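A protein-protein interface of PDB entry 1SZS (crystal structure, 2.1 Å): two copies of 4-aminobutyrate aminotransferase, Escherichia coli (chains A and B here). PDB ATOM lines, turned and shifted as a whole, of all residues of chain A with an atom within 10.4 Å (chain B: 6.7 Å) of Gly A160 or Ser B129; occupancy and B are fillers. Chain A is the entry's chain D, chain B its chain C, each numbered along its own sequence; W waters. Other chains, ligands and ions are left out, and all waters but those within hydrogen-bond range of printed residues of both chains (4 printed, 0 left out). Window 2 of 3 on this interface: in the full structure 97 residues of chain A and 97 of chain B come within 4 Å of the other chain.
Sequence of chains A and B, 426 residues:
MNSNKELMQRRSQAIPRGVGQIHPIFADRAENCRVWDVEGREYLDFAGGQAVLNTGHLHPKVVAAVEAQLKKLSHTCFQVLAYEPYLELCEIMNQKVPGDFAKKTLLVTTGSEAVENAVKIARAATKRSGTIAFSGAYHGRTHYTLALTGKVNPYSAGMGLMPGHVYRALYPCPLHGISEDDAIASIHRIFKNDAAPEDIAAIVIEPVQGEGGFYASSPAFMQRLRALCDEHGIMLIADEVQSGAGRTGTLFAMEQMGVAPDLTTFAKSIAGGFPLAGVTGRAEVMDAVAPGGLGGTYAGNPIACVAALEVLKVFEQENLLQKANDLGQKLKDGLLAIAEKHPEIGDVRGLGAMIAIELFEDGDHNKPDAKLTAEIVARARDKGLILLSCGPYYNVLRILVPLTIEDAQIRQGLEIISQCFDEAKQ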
ATOM      1  N   THR A 142      10.341  13.328   8.731  1.00  0.00           N
ATOM      2  CA  THR A 142       8.914  13.319   8.446  1.00  0.00           C
ATOM      3  C   THR A 142       8.388  12.078   9.180  1.00  0.00           C
ATOM      4  O   THR A 142       9.191  11.208   9.544  1.00  0.00           O
ATOM      5  CB  THR A 142       8.625  13.168   6.927  1.00  0.00           C
ATOM      6  OG1 THR A 142       9.257  11.976   6.428  1.00  0.00           O
ATOM      7  CG2 THR A 142       9.140  14.369   6.177  1.00  0.00           C
ATOM      8  N   HIS A 143       7.073  11.980   9.391  1.00  0.00           N
ATOM      9  CA  HIS A 143       6.535  10.826  10.107  1.00  0.00           C
ATOM     10  C   HIS A 143       7.106   9.500   9.587  1.00  0.00           C
ATOM     11  O   HIS A 143       7.639   8.720  10.359  1.00  0.00           O
ATOM     12  CB  HIS A 143       4.999  10.759  10.022  1.00  0.00           C
ATOM     13  CG  HIS A 143       4.293  11.639  11.010  1.00  0.00           C
ATOM     14  ND1 HIS A 143       4.257  13.011  10.902  1.00  0.00           N
ATOM     15  CD2 HIS A 143       3.600  11.331  12.131  1.00  0.00           C
ATOM     16  CE1 HIS A 143       3.568  13.513  11.912  1.00  0.00           C
ATOM     17  NE2 HIS A 143       3.159  12.513  12.674  1.00  0.00           N
ATOM     18  N   LEU A 146      10.853   9.067  10.031  1.00  0.00           N
ATOM     19  CA  LEU A 146      11.199   8.902  11.450  1.00  0.00           C
ATOM     20  C   LEU A 146      10.970   7.410  11.827  1.00  0.00           C
ATOM     21  O   LEU A 146      11.672   6.869  12.688  1.00  0.00           O
ATOM     22  CB  LEU A 146      10.354   9.829  12.340  1.00  0.00           C
ATOM     23  CG  LEU A 146      10.763  11.313  12.364  1.00  0.00           C
ATOM     24  CD1 LEU A 146       9.795  12.083  13.232  1.00  0.00           C
ATOM     25  CD2 LEU A 146      12.159  11.470  12.900  1.00  0.00           C
ATOM     26  N   ALA A 147       9.999   6.755  11.178  1.00  0.00           N
ATOM     27  CA  ALA A 147       9.747   5.325  11.415  1.00  0.00           C
ATOM     28  C   ALA A 147      10.953   4.564  10.841  1.00  0.00           C
ATOM     29  O   ALA A 147      11.458   3.646  11.489  1.00  0.00           O
ATOM     30  CB  ALA A 147       8.470   4.867  10.705  1.00  0.00           C
ATOM     31  N   LYS A 151      16.234   5.278  15.518  1.00  0.00           N
ATOM     32  CA  LYS A 151      16.546   6.038  16.725  1.00  0.00           C
ATOM     33  C   LYS A 151      15.305   6.880  17.026  1.00  0.00           C
ATOM     34  O   LYS A 151      14.919   7.751  16.227  1.00  0.00           O
ATOM     35  CB  LYS A 151      17.750   6.951  16.482  1.00  0.00           C
ATOM     36  CG  LYS A 151      18.204   7.723  17.707  1.00  0.00           C
ATOM     37  CD  LYS A 151      19.586   8.320  17.478  1.00  0.00           C
ATOM     38  CE  LYS A 151      20.097   9.098  18.697  1.00  0.00           C
ATOM     39  NZ  LYS A 151      20.322   8.210  19.869  1.00  0.00           N
ATOM     40  N   VAL A 152      14.675   6.588  18.151  1.00  0.00           N
ATOM     41  CA  VAL A 152      13.460   7.274  18.578  1.00  0.00           C
ATOM     42  C   VAL A 152      13.759   8.624  19.263  1.00  0.00           C
ATOM     43  O   VAL A 152      13.127   9.644  18.958  1.00  0.00           O
ATOM     44  CB  VAL A 152      12.670   6.395  19.569  1.00  0.00           C
ATOM     45  CG1 VAL A 152      11.391   7.096  19.973  1.00  0.00           C
ATOM     46  CG2 VAL A 152      12.377   5.042  18.937  1.00  0.00           C
ATOM     47  N   ASN A 153      14.723   8.616  20.180  1.00  0.00           N
ATOM     48  CA  ASN A 153      15.096   9.826  20.897  1.00  0.00           C
ATOM     49  C   ASN A 153      16.355  10.454  20.300  1.00  0.00           C
ATOM     50  O   ASN A 153      17.385   9.797  20.163  1.00  0.00           O
ATOM     51  CB  ASN A 153      15.313   9.507  22.376  1.00  0.00           C
ATOM     52  CG  ASN A 153      15.718  10.729  23.179  1.00  0.00           C
ATOM     53  OD1 ASN A 153      15.156  11.809  23.004  1.00  0.00           O
ATOM     54  ND2 ASN A 153      16.691  10.563  24.070  1.00  0.00           N
ATOM     55  N   PRO A 154      16.300  11.751  19.980  1.00  0.00           N
ATOM     56  CA  PRO A 154      15.164  12.667  20.142  1.00  0.00           C
ATOM     57  C   PRO A 154      14.271  12.855  18.912  1.00  0.00           C
ATOM     58  O   PRO A 154      13.200  13.459  19.034  1.00  0.00           O
ATOM     59  CB  PRO A 154      15.853  13.971  20.473  1.00  0.00           C
ATOM     60  CG  PRO A 154      16.983  13.958  19.424  1.00  0.00           C
ATOM     61  CD  PRO A 154      17.465  12.476  19.436  1.00  0.00           C
ATOM     62  N   TYR A 155      14.731  12.386  17.749  1.00  0.00           N
ATOM     63  CA  TYR A 155      14.016  12.554  16.478  1.00  0.00           C
ATOM     64  C   TYR A 155      12.495  12.431  16.540  1.00  0.00           C
ATOM     65  O   TYR A 155      11.799  13.223  15.911  1.00  0.00           O
ATOM     66  CB  TYR A 155      14.597  11.593  15.442  1.00  0.00           C
ATOM     67  CG  TYR A 155      16.101  11.705  15.355  1.00  0.00           C
ATOM     68  CD1 TYR A 155      16.900  10.576  15.340  1.00  0.00           C
ATOM     69  CD2 TYR A 155      16.726  12.954  15.354  1.00  0.00           C
ATOM     70  CE1 TYR A 155      18.282  10.676  15.333  1.00  0.00           C
ATOM     71  CE2 TYR A 155      18.101  13.071  15.345  1.00  0.00           C
ATOM     72  CZ  TYR A 155      18.880  11.925  15.335  1.00  0.00           C
ATOM     73  OH  TYR A 155      20.258  12.031  15.322  1.00  0.00           O
ATOM     74  N   SER A 156      11.969  11.469  17.290  1.00  0.00           N
ATOM     75  CA  SER A 156      10.518  11.322  17.383  1.00  0.00           C
ATOM     76  C   SER A 156      10.041  11.113  18.822  1.00  0.00           C
ATOM     77  O   SER A 156       8.989  10.527  19.062  1.00  0.00           O
ATOM     78  CB  SER A 156      10.015  10.182  16.454  1.00  0.00           C
ATOM     79  OG  SER A 156      10.640   8.924  16.696  1.00  0.00           O
ATOM     80  N   ALA A 157      10.823  11.625  19.768  1.00  0.00           N
ATOM     81  CA  ALA A 157      10.517  11.523  21.202  1.00  0.00           C
ATOM     82  C   ALA A 157       9.251  12.288  21.608  1.00  0.00           C
ATOM     83  O   ALA A 157       9.013  13.404  21.144  1.00  0.00           O
ATOM     84  CB  ALA A 157      11.707  12.037  22.016  1.00  0.00           C
ATOM     85  N   GLY A 158       8.446  11.672  22.466  1.00  0.00           N
ATOM     86  CA  GLY A 158       7.227  12.291  22.958  1.00  0.00           C
ATOM     87  C   GLY A 158       6.069  12.448  21.991  1.00  0.00           C
ATOM     88  O   GLY A 158       5.026  12.992  22.363  1.00  0.00           O
ATOM     89  N   MET A 159       6.205  11.972  20.760  1.00  0.00           N
ATOM     90  CA  MET A 159       5.109  12.156  19.806  1.00  0.00           C
ATOM     91  C   MET A 159       4.179  10.941  19.648  1.00  0.00           C
ATOM     92  O   MET A 159       3.219  11.014  18.890  1.00  0.00           O
ATOM     93  CB  MET A 159       5.684  12.530  18.440  1.00  0.00           C
ATOM     94  CG  MET A 159       6.615  13.731  18.467  1.00  0.00           C
ATOM     95  SD  MET A 159       7.649  13.825  17.000  1.00  0.00           S
ATOM     96  CE  MET A 159       9.120  14.620  17.557  1.00  0.00           C
ATOM     97  N   GLY A 160       4.445   9.851  20.365  1.00  0.00           N
ATOM     98  CA  GLY A 160       3.627   8.658  20.206  1.00  0.00           C
ATOM     99  C   GLY A 160       4.292   7.785  19.129  1.00  0.00           C
ATOM    100  O   GLY A 160       5.345   8.154  18.601  1.00  0.00           O
ATOM    101  N   LEU A 161       3.682   6.650  18.786  1.00  0.00           N
ATOM    102  CA  LEU A 161       4.248   5.734  17.796  1.00  0.00           C
ATOM    103  C   LEU A 161       4.213   6.275  16.353  1.00  0.00           C
ATOM    104  O   LEU A 161       3.191   6.818  15.913  1.00  0.00           O
ATOM    105  CB  LEU A 161       3.530   4.383  17.867  1.00  0.00           C
ATOM    106  CG  LEU A 161       3.747   3.616  19.174  1.00  0.00           C
ATOM    107  CD1 LEU A 161       2.827   2.425  19.187  1.00  0.00           C
ATOM    108  CD2 LEU A 161       5.215   3.197  19.337  1.00  0.00           C
ATOM    109  N   MET A 162       5.335   6.138  15.637  1.00  0.00           N
ATOM    110  CA  MET A 162       5.431   6.604  14.247  1.00  0.00           C
ATOM    111  C   MET A 162       4.773   5.527  13.346  1.00  0.00           C
ATOM    112  O   MET A 162       4.513   4.411  13.808  1.00  0.00           O
ATOM    113  CB  MET A 162       6.897   6.823  13.868  1.00  0.00           C
ATOM    114  CG  MET A 162       7.545   8.056  14.516  1.00  0.00           C
ATOM    115  SD  MET A 162       6.671   9.565  14.023  1.00  0.00           S
ATOM    116  CE  MET A 162       5.646   9.891  15.570  1.00  0.00           C
ATOM    117  N   PRO A 163       4.482   5.850  12.081  1.00  0.00           N
ATOM    118  CA  PRO A 163       3.849   4.893  11.162  1.00  0.00           C
ATOM    119  C   PRO A 163       4.345   3.457  11.257  1.00  0.00           C
ATOM    120  O   PRO A 163       5.537   3.194  11.440  1.00  0.00           O
ATOM    121  CB  PRO A 163       4.101   5.522   9.801  1.00  0.00           C
ATOM    122  CG  PRO A 163       3.912   6.981  10.127  1.00  0.00           C
ATOM    123  CD  PRO A 163       4.766   7.116  11.380  1.00  0.00           C
ATOM    124  N   GLY A 164       3.412   2.530  11.147  1.00  0.00           N
ATOM    125  CA  GLY A 164       3.769   1.134  11.229  1.00  0.00           C
ATOM    126  C   GLY A 164       4.191   0.548   9.898  1.00  0.00           C
ATOM    127  O   GLY A 164       4.304   1.256   8.883  1.00  0.00           O
ATOM    128  N   VAL B 119       1.918  18.808  12.872  1.00  0.00           N
ATOM    129  CA  VAL B 119       1.283  17.601  13.439  1.00  0.00           C
ATOM    130  C   VAL B 119       2.181  16.976  14.552  1.00  0.00           C
ATOM    131  O   VAL B 119       1.705  16.638  15.649  1.00  0.00           O
ATOM    132  CB  VAL B 119       0.994  16.538  12.343  1.00  0.00           C
ATOM    133  CG1 VAL B 119       0.507  15.229  12.998  1.00  0.00           C
ATOM    134  CG2 VAL B 119      -0.105  17.049  11.409  1.00  0.00           C
ATOM    135  N   ARG B 123       1.083  16.563  18.381  1.00  0.00           N
ATOM    136  CA  ARG B 123       1.052  15.264  19.024  1.00  0.00           C
ATOM    137  C   ARG B 123       1.855  15.342  20.310  1.00  0.00           C
ATOM    138  O   ARG B 123       1.413  14.835  21.327  1.00  0.00           O
ATOM    139  CB  ARG B 123       1.604  14.172  18.095  1.00  0.00           C
ATOM    140  CG  ARG B 123       0.663  13.886  16.926  1.00  0.00           C
ATOM    141  CD  ARG B 123       1.234  12.874  15.959  1.00  0.00           C
ATOM    142  NE  ARG B 123       1.536  11.599  16.604  1.00  0.00           N
ATOM    143  CZ  ARG B 123       1.787  10.477  15.935  1.00  0.00           C
ATOM    144  NH1 ARG B 123       1.774  10.483  14.600  1.00  0.00           N
ATOM    145  NH2 ARG B 123       2.022   9.341  16.596  1.00  0.00           N
ATOM    146  N   ALA B 124       3.015  15.988  20.266  1.00  0.00           N
ATOM    147  CA  ALA B 124       3.846  16.112  21.463  1.00  0.00           C
ATOM    148  C   ALA B 124       3.136  16.993  22.544  1.00  0.00           C
ATOM    149  O   ALA B 124       3.171  16.684  23.726  1.00  0.00           O
ATOM    150  CB  ALA B 124       5.212  16.709  21.097  1.00  0.00           C
ATOM    151  N   THR B 126      -0.196  17.482  23.035  1.00  0.00           N
ATOM    152  CA  THR B 126      -1.393  16.853  23.577  1.00  0.00           C
ATOM    153  C   THR B 126      -1.193  15.411  24.052  1.00  0.00           C
ATOM    154  O   THR B 126      -2.037  14.883  24.785  1.00  0.00           O
ATOM    155  CB  THR B 126      -2.537  16.817  22.523  1.00  0.00           C
ATOM    156  OG1 THR B 126      -2.109  16.052  21.379  1.00  0.00           O
ATOM    157  CG2 THR B 126      -2.938  18.223  22.090  1.00  0.00           C
ATOM    158  N   LYS B 127      -0.107  14.784  23.613  1.00  0.00           N
ATOM    159  CA  LYS B 127       0.178  13.403  23.970  1.00  0.00           C
ATOM    160  C   LYS B 127      -0.898  12.521  23.358  1.00  0.00           C
ATOM    161  O   LYS B 127      -1.395  11.600  24.002  1.00  0.00           O
ATOM    162  CB  LYS B 127       0.185  13.225  25.480  1.00  0.00           C
ATOM    163  CG  LYS B 127       1.172  14.137  26.194  1.00  0.00           C
ATOM    164  CD  LYS B 127       2.496  13.462  26.431  1.00  0.00           C
ATOM    165  CE  LYS B 127       3.315  14.228  27.465  1.00  0.00           C
ATOM    166  NZ  LYS B 127       4.639  13.559  27.695  1.00  0.00           N
ATOM    167  N   ARG B 128      -1.243  12.825  22.110  1.00  0.00           N
ATOM    168  CA  ARG B 128      -2.256  12.092  21.356  1.00  0.00           C
ATOM    169  C   ARG B 128      -1.639  11.760  19.994  1.00  0.00           C
ATOM    170  O   ARG B 128      -0.762  12.484  19.544  1.00  0.00           O
ATOM    171  CB  ARG B 128      -3.487  12.964  21.169  1.00  0.00           C
ATOM    172  CG  ARG B 128      -4.118  13.360  22.476  1.00  0.00           C
ATOM    173  CD  ARG B 128      -5.361  14.199  22.240  1.00  0.00           C
ATOM    174  NE  ARG B 128      -5.841  14.773  23.481  1.00  0.00           N
ATOM    175  CZ  ARG B 128      -6.764  15.726  23.547  1.00  0.00           C
ATOM    176  NH1 ARG B 128      -7.299  16.206  22.432  1.00  0.00           N
ATOM    177  NH2 ARG B 128      -7.153  16.195  24.736  1.00  0.00           N
ATOM    178  N   SER B 129      -2.099  10.689  19.350  1.00  0.00           N
ATOM    179  CA  SER B 129      -1.538  10.278  18.071  1.00  0.00           C
ATOM    180  C   SER B 129      -2.402  10.491  16.830  1.00  0.00           C
ATOM    181  O   SER B 129      -1.886  10.422  15.720  1.00  0.00           O
ATOM    182  CB  SER B 129      -1.151   8.801  18.136  1.00  0.00           C
ATOM    183  OG  SER B 129      -0.032   8.604  18.987  1.00  0.00           O
ATOM    184  N   GLY B 130      -3.689  10.756  17.006  1.00  0.00           N
ATOM    185  CA  GLY B 130      -4.548  10.892  15.850  1.00  0.00           C
ATOM    186  C   GLY B 130      -4.791  12.306  15.382  1.00  0.00           C
ATOM    187  O   GLY B 130      -4.632  13.265  16.147  1.00  0.00           O
ATOM    188  N   THR B 131      -5.179  12.428  14.117  1.00  0.00           N
ATOM    189  CA  THR B 131      -5.489  13.714  13.527  1.00  0.00           C
ATOM    190  C   THR B 131      -6.723  13.577  12.625  1.00  0.00           C
ATOM    191  O   THR B 131      -7.082  12.461  12.197  1.00  0.00           O
ATOM    192  CB  THR B 131      -4.303  14.256  12.690  1.00  0.00           C
ATOM    193  OG1 THR B 131      -4.042  13.382  11.593  1.00  0.00           O
ATOM    194  CG2 THR B 131      -3.068  14.338  13.526  1.00  0.00           C
ATOM    195  N   TYR B 144       2.616  10.761   5.302  1.00  0.00           N
ATOM    196  CA  TYR B 144       1.632  11.265   6.239  1.00  0.00           C
ATOM    197  C   TYR B 144       0.796  12.415   5.674  1.00  0.00           C
ATOM    198  O   TYR B 144      -0.399  12.437   5.911  1.00  0.00           O
ATOM    199  CB  TYR B 144       2.297  11.676   7.563  1.00  0.00           C
ATOM    200  CG  TYR B 144       1.289  11.836   8.684  1.00  0.00           C
ATOM    201  CD1 TYR B 144       0.871  10.736   9.438  1.00  0.00           C
ATOM    202  CD2 TYR B 144       0.727  13.072   8.963  1.00  0.00           C
ATOM    203  CE1 TYR B 144      -0.092  10.861  10.452  1.00  0.00           C
ATOM    204  CE2 TYR B 144      -0.245  13.214   9.981  1.00  0.00           C
ATOM    205  CZ  TYR B 144      -0.647  12.100  10.716  1.00  0.00           C
ATOM    206  OH  TYR B 144      -1.605  12.228  11.703  1.00  0.00           O
ATOM    207  N   GLY B 164      -2.350   5.030   8.636  1.00  0.00           N
ATOM    208  CA  GLY B 164      -3.651   5.063   9.278  1.00  0.00           C
ATOM    209  C   GLY B 164      -3.718   6.120  10.372  1.00  0.00           C
ATOM    210  O   GLY B 164      -2.794   6.921  10.571  1.00  0.00           O
ATOM    211  N   HIS B 165      -4.828   6.121  11.089  1.00  0.00           N
ATOM    212  CA  HIS B 165      -5.021   7.046  12.185  1.00  0.00           C
ATOM    213  C   HIS B 165      -5.137   8.512  11.799  1.00  0.00           C
ATOM    214  O   HIS B 165      -4.778   9.397  12.572  1.00  0.00           O
ATOM    215  CB  HIS B 165      -3.940   6.796  13.244  1.00  0.00           C
ATOM    216  CG  HIS B 165      -4.057   5.438  13.864  1.00  0.00           C
ATOM    217  ND1 HIS B 165      -3.085   4.887  14.667  1.00  0.00           N
ATOM    218  CD2 HIS B 165      -5.034   4.504  13.761  1.00  0.00           C
ATOM    219  CE1 HIS B 165      -3.456   3.671  15.032  1.00  0.00           C
ATOM    220  NE2 HIS B 165      -4.635   3.414  14.493  1.00  0.00           N
ATOM    221  N   VAL B 166      -5.658   8.734  10.595  1.00  0.00           N
ATOM    222  CA  VAL B 166      -5.956  10.054  10.060  1.00  0.00           C
ATOM    223  C   VAL B 166      -7.432   9.888   9.686  1.00  0.00           C
ATOM    224  O   VAL B 166      -7.762   8.993   8.892  1.00  0.00           O
ATOM    225  CB  VAL B 166      -5.129  10.379   8.807  1.00  0.00           C
ATOM    226  CG1 VAL B 166      -5.764  11.567   8.050  1.00  0.00           C
ATOM    227  CG2 VAL B 166      -3.710  10.741   9.215  1.00  0.00           C
ATOM    228  N   GLU B 198     -10.052  12.340  23.056  1.00  0.00           N
ATOM    229  CA  GLU B 198      -8.832  12.082  23.821  1.00  0.00           C
ATOM    230  C   GLU B 198      -7.713  11.465  22.957  1.00  0.00           C
ATOM    231  O   GLU B 198      -6.579  11.378  23.414  1.00  0.00           O
ATOM    232  CB  GLU B 198      -9.133  11.144  24.999  1.00  0.00           C
ATOM    233  CG  GLU B 198      -9.496   9.741  24.568  1.00  0.00           C
ATOM    234  CD  GLU B 198     -10.212   8.933  25.649  1.00  0.00           C
ATOM    235  OE1 GLU B 198     -11.355   9.300  26.005  1.00  0.00           O
ATOM    236  OE2 GLU B 198      -9.646   7.926  26.132  1.00  0.00           O
ATOM    237  N   ASP B 199      -8.022  11.016  21.739  1.00  0.00           N
ATOM    238  CA  ASP B 199      -6.975  10.450  20.880  1.00  0.00           C
ATOM    239  C   ASP B 199      -6.732  11.323  19.666  1.00  0.00           C
ATOM    240  O   ASP B 199      -5.993  10.925  18.760  1.00  0.00           O
ATOM    241  CB  ASP B 199      -7.317   9.021  20.422  1.00  0.00           C
ATOM    242  CG  ASP B 199      -7.173   8.006  21.539  1.00  0.00           C
ATOM    243  OD1 ASP B 199      -8.161   7.333  21.878  1.00  0.00           O
ATOM    244  OD2 ASP B 199      -6.056   7.876  22.078  1.00  0.00           O
ATOM    245  N   ILE B 200      -7.343  12.503  19.631  1.00  0.00           N
ATOM    246  CA  ILE B 200      -7.127  13.404  18.496  1.00  0.00           C
ATOM    247  C   ILE B 200      -6.228  14.597  18.912  1.00  0.00           C
ATOM    248  O   ILE B 200      -6.629  15.432  19.708  1.00  0.00           O
ATOM    249  CB  ILE B 200      -8.473  13.930  17.941  1.00  0.00           C
ATOM    250  CG1 ILE B 200      -9.312  12.759  17.422  1.00  0.00           C
ATOM    251  CG2 ILE B 200      -8.237  14.939  16.830  1.00  0.00           C
ATOM    252  CD1 ILE B 200      -8.646  11.939  16.310  1.00  0.00           C
ATOM    253  N   ALA B 201      -5.016  14.651  18.375  1.00  0.00           N
ATOM    254  CA  ALA B 201      -4.075  15.720  18.695  1.00  0.00           C
ATOM    255  C   ALA B 201      -4.361  17.013  17.938  1.00  0.00           C
ATOM    256  O   ALA B 201      -4.107  18.117  18.451  1.00  0.00           O
ATOM    257  CB  ALA B 201      -2.678  15.265  18.384  1.00  0.00           C
HETATM  258  O   HOH W   1       5.178  14.953  24.566  1.00  0.00           O
HETATM  259  O   HOH W   2       2.645  12.255  22.235  1.00  0.00           O
HETATM  260  O   HOH W   3       2.326   7.993  13.263  1.00  0.00           O
HETATM  261  O   HOH W   4       0.937   6.015  19.968  1.00  0.00           O
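Gly A160 touches just these residues of chain B: Arg B123 (3.7 Å) and Ser B129 (3.9 Å). Of the printed residues of chain B, Leu A161 touches Arg B123. Of the printed residues of chain A, Ala B124 touches Gly A158. Ser B129 touches just one residue of chain A: Gly A160 (3.9 Å). No residue of chain A comes within 4 Å of Gly B130. The nearest printed residue of chain A that does not touch Arg B123 is Gly A158 (4.2 Å).
Hydrophobic or aromatic side chains of chain B that line the printed part of chain A: Val B119, Ala B124 and Tyr B144. Among the printed residues, no Asp or Glu carboxylate lies within 4 Å of a Lys or Arg side-chain nitrogen of the other chain.
Water W2 bridges O of Gly A158 (2.5 Å) and O of Arg B123 (3.0 Å). Water W1 lies within hydrogen-bond range of the backbone carbonyl oxygen of Ala B124, the backbone carbonyl oxygen of Gly A158 and the side-chain amino group of Lys B127. Water W3 bridges NH1 of Arg B123 (2.9 Å) and O of Leu A161 (3.0 Å). Water W4 lies within hydrogen-bond range of the side-chain hydroxyl of Ser B129 (2.9 Å) and the backbone NH of Leu A161 (3.1 Å).
Among the printed residues, merely in contact across the chains: Gly A158 with Ala B124 (3.5 Å), His A143 with Val B119 (3.7 Å), Gly A160 with Arg B123 (3.7 Å), His A143 with Tyr B144 (3.8 Å), Met A162 with Arg B123 (3.8 Å) and Gly A160 with Ser B129 (3.9 Å).
The guanidinium group (NH1) of Arg B123 lies within hydrogen-bond range of a ring nitrogen (NE2) of His A143 (3.1 Å). NE of Arg B123 is in hydrogen-bond range of O of Met A159 (2.9 Å). NH2 of Arg B123 is in hydrogen-bond range of O of Leu A161, at 2.9 Å.
Position printed for both chains: 164.
O of Arg B123 is in hydrogen-bond range of N of Arg B128, 3.4 Å away. OG of Ser B129 lies within hydrogen-bond range of NH2 of Arg B123 (3.2 Å). The side-chain hydroxyl of Thr B131 sits at hydrogen-bond distance from the side-chain hydroxyl of Tyr B144 (2.7 Å).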
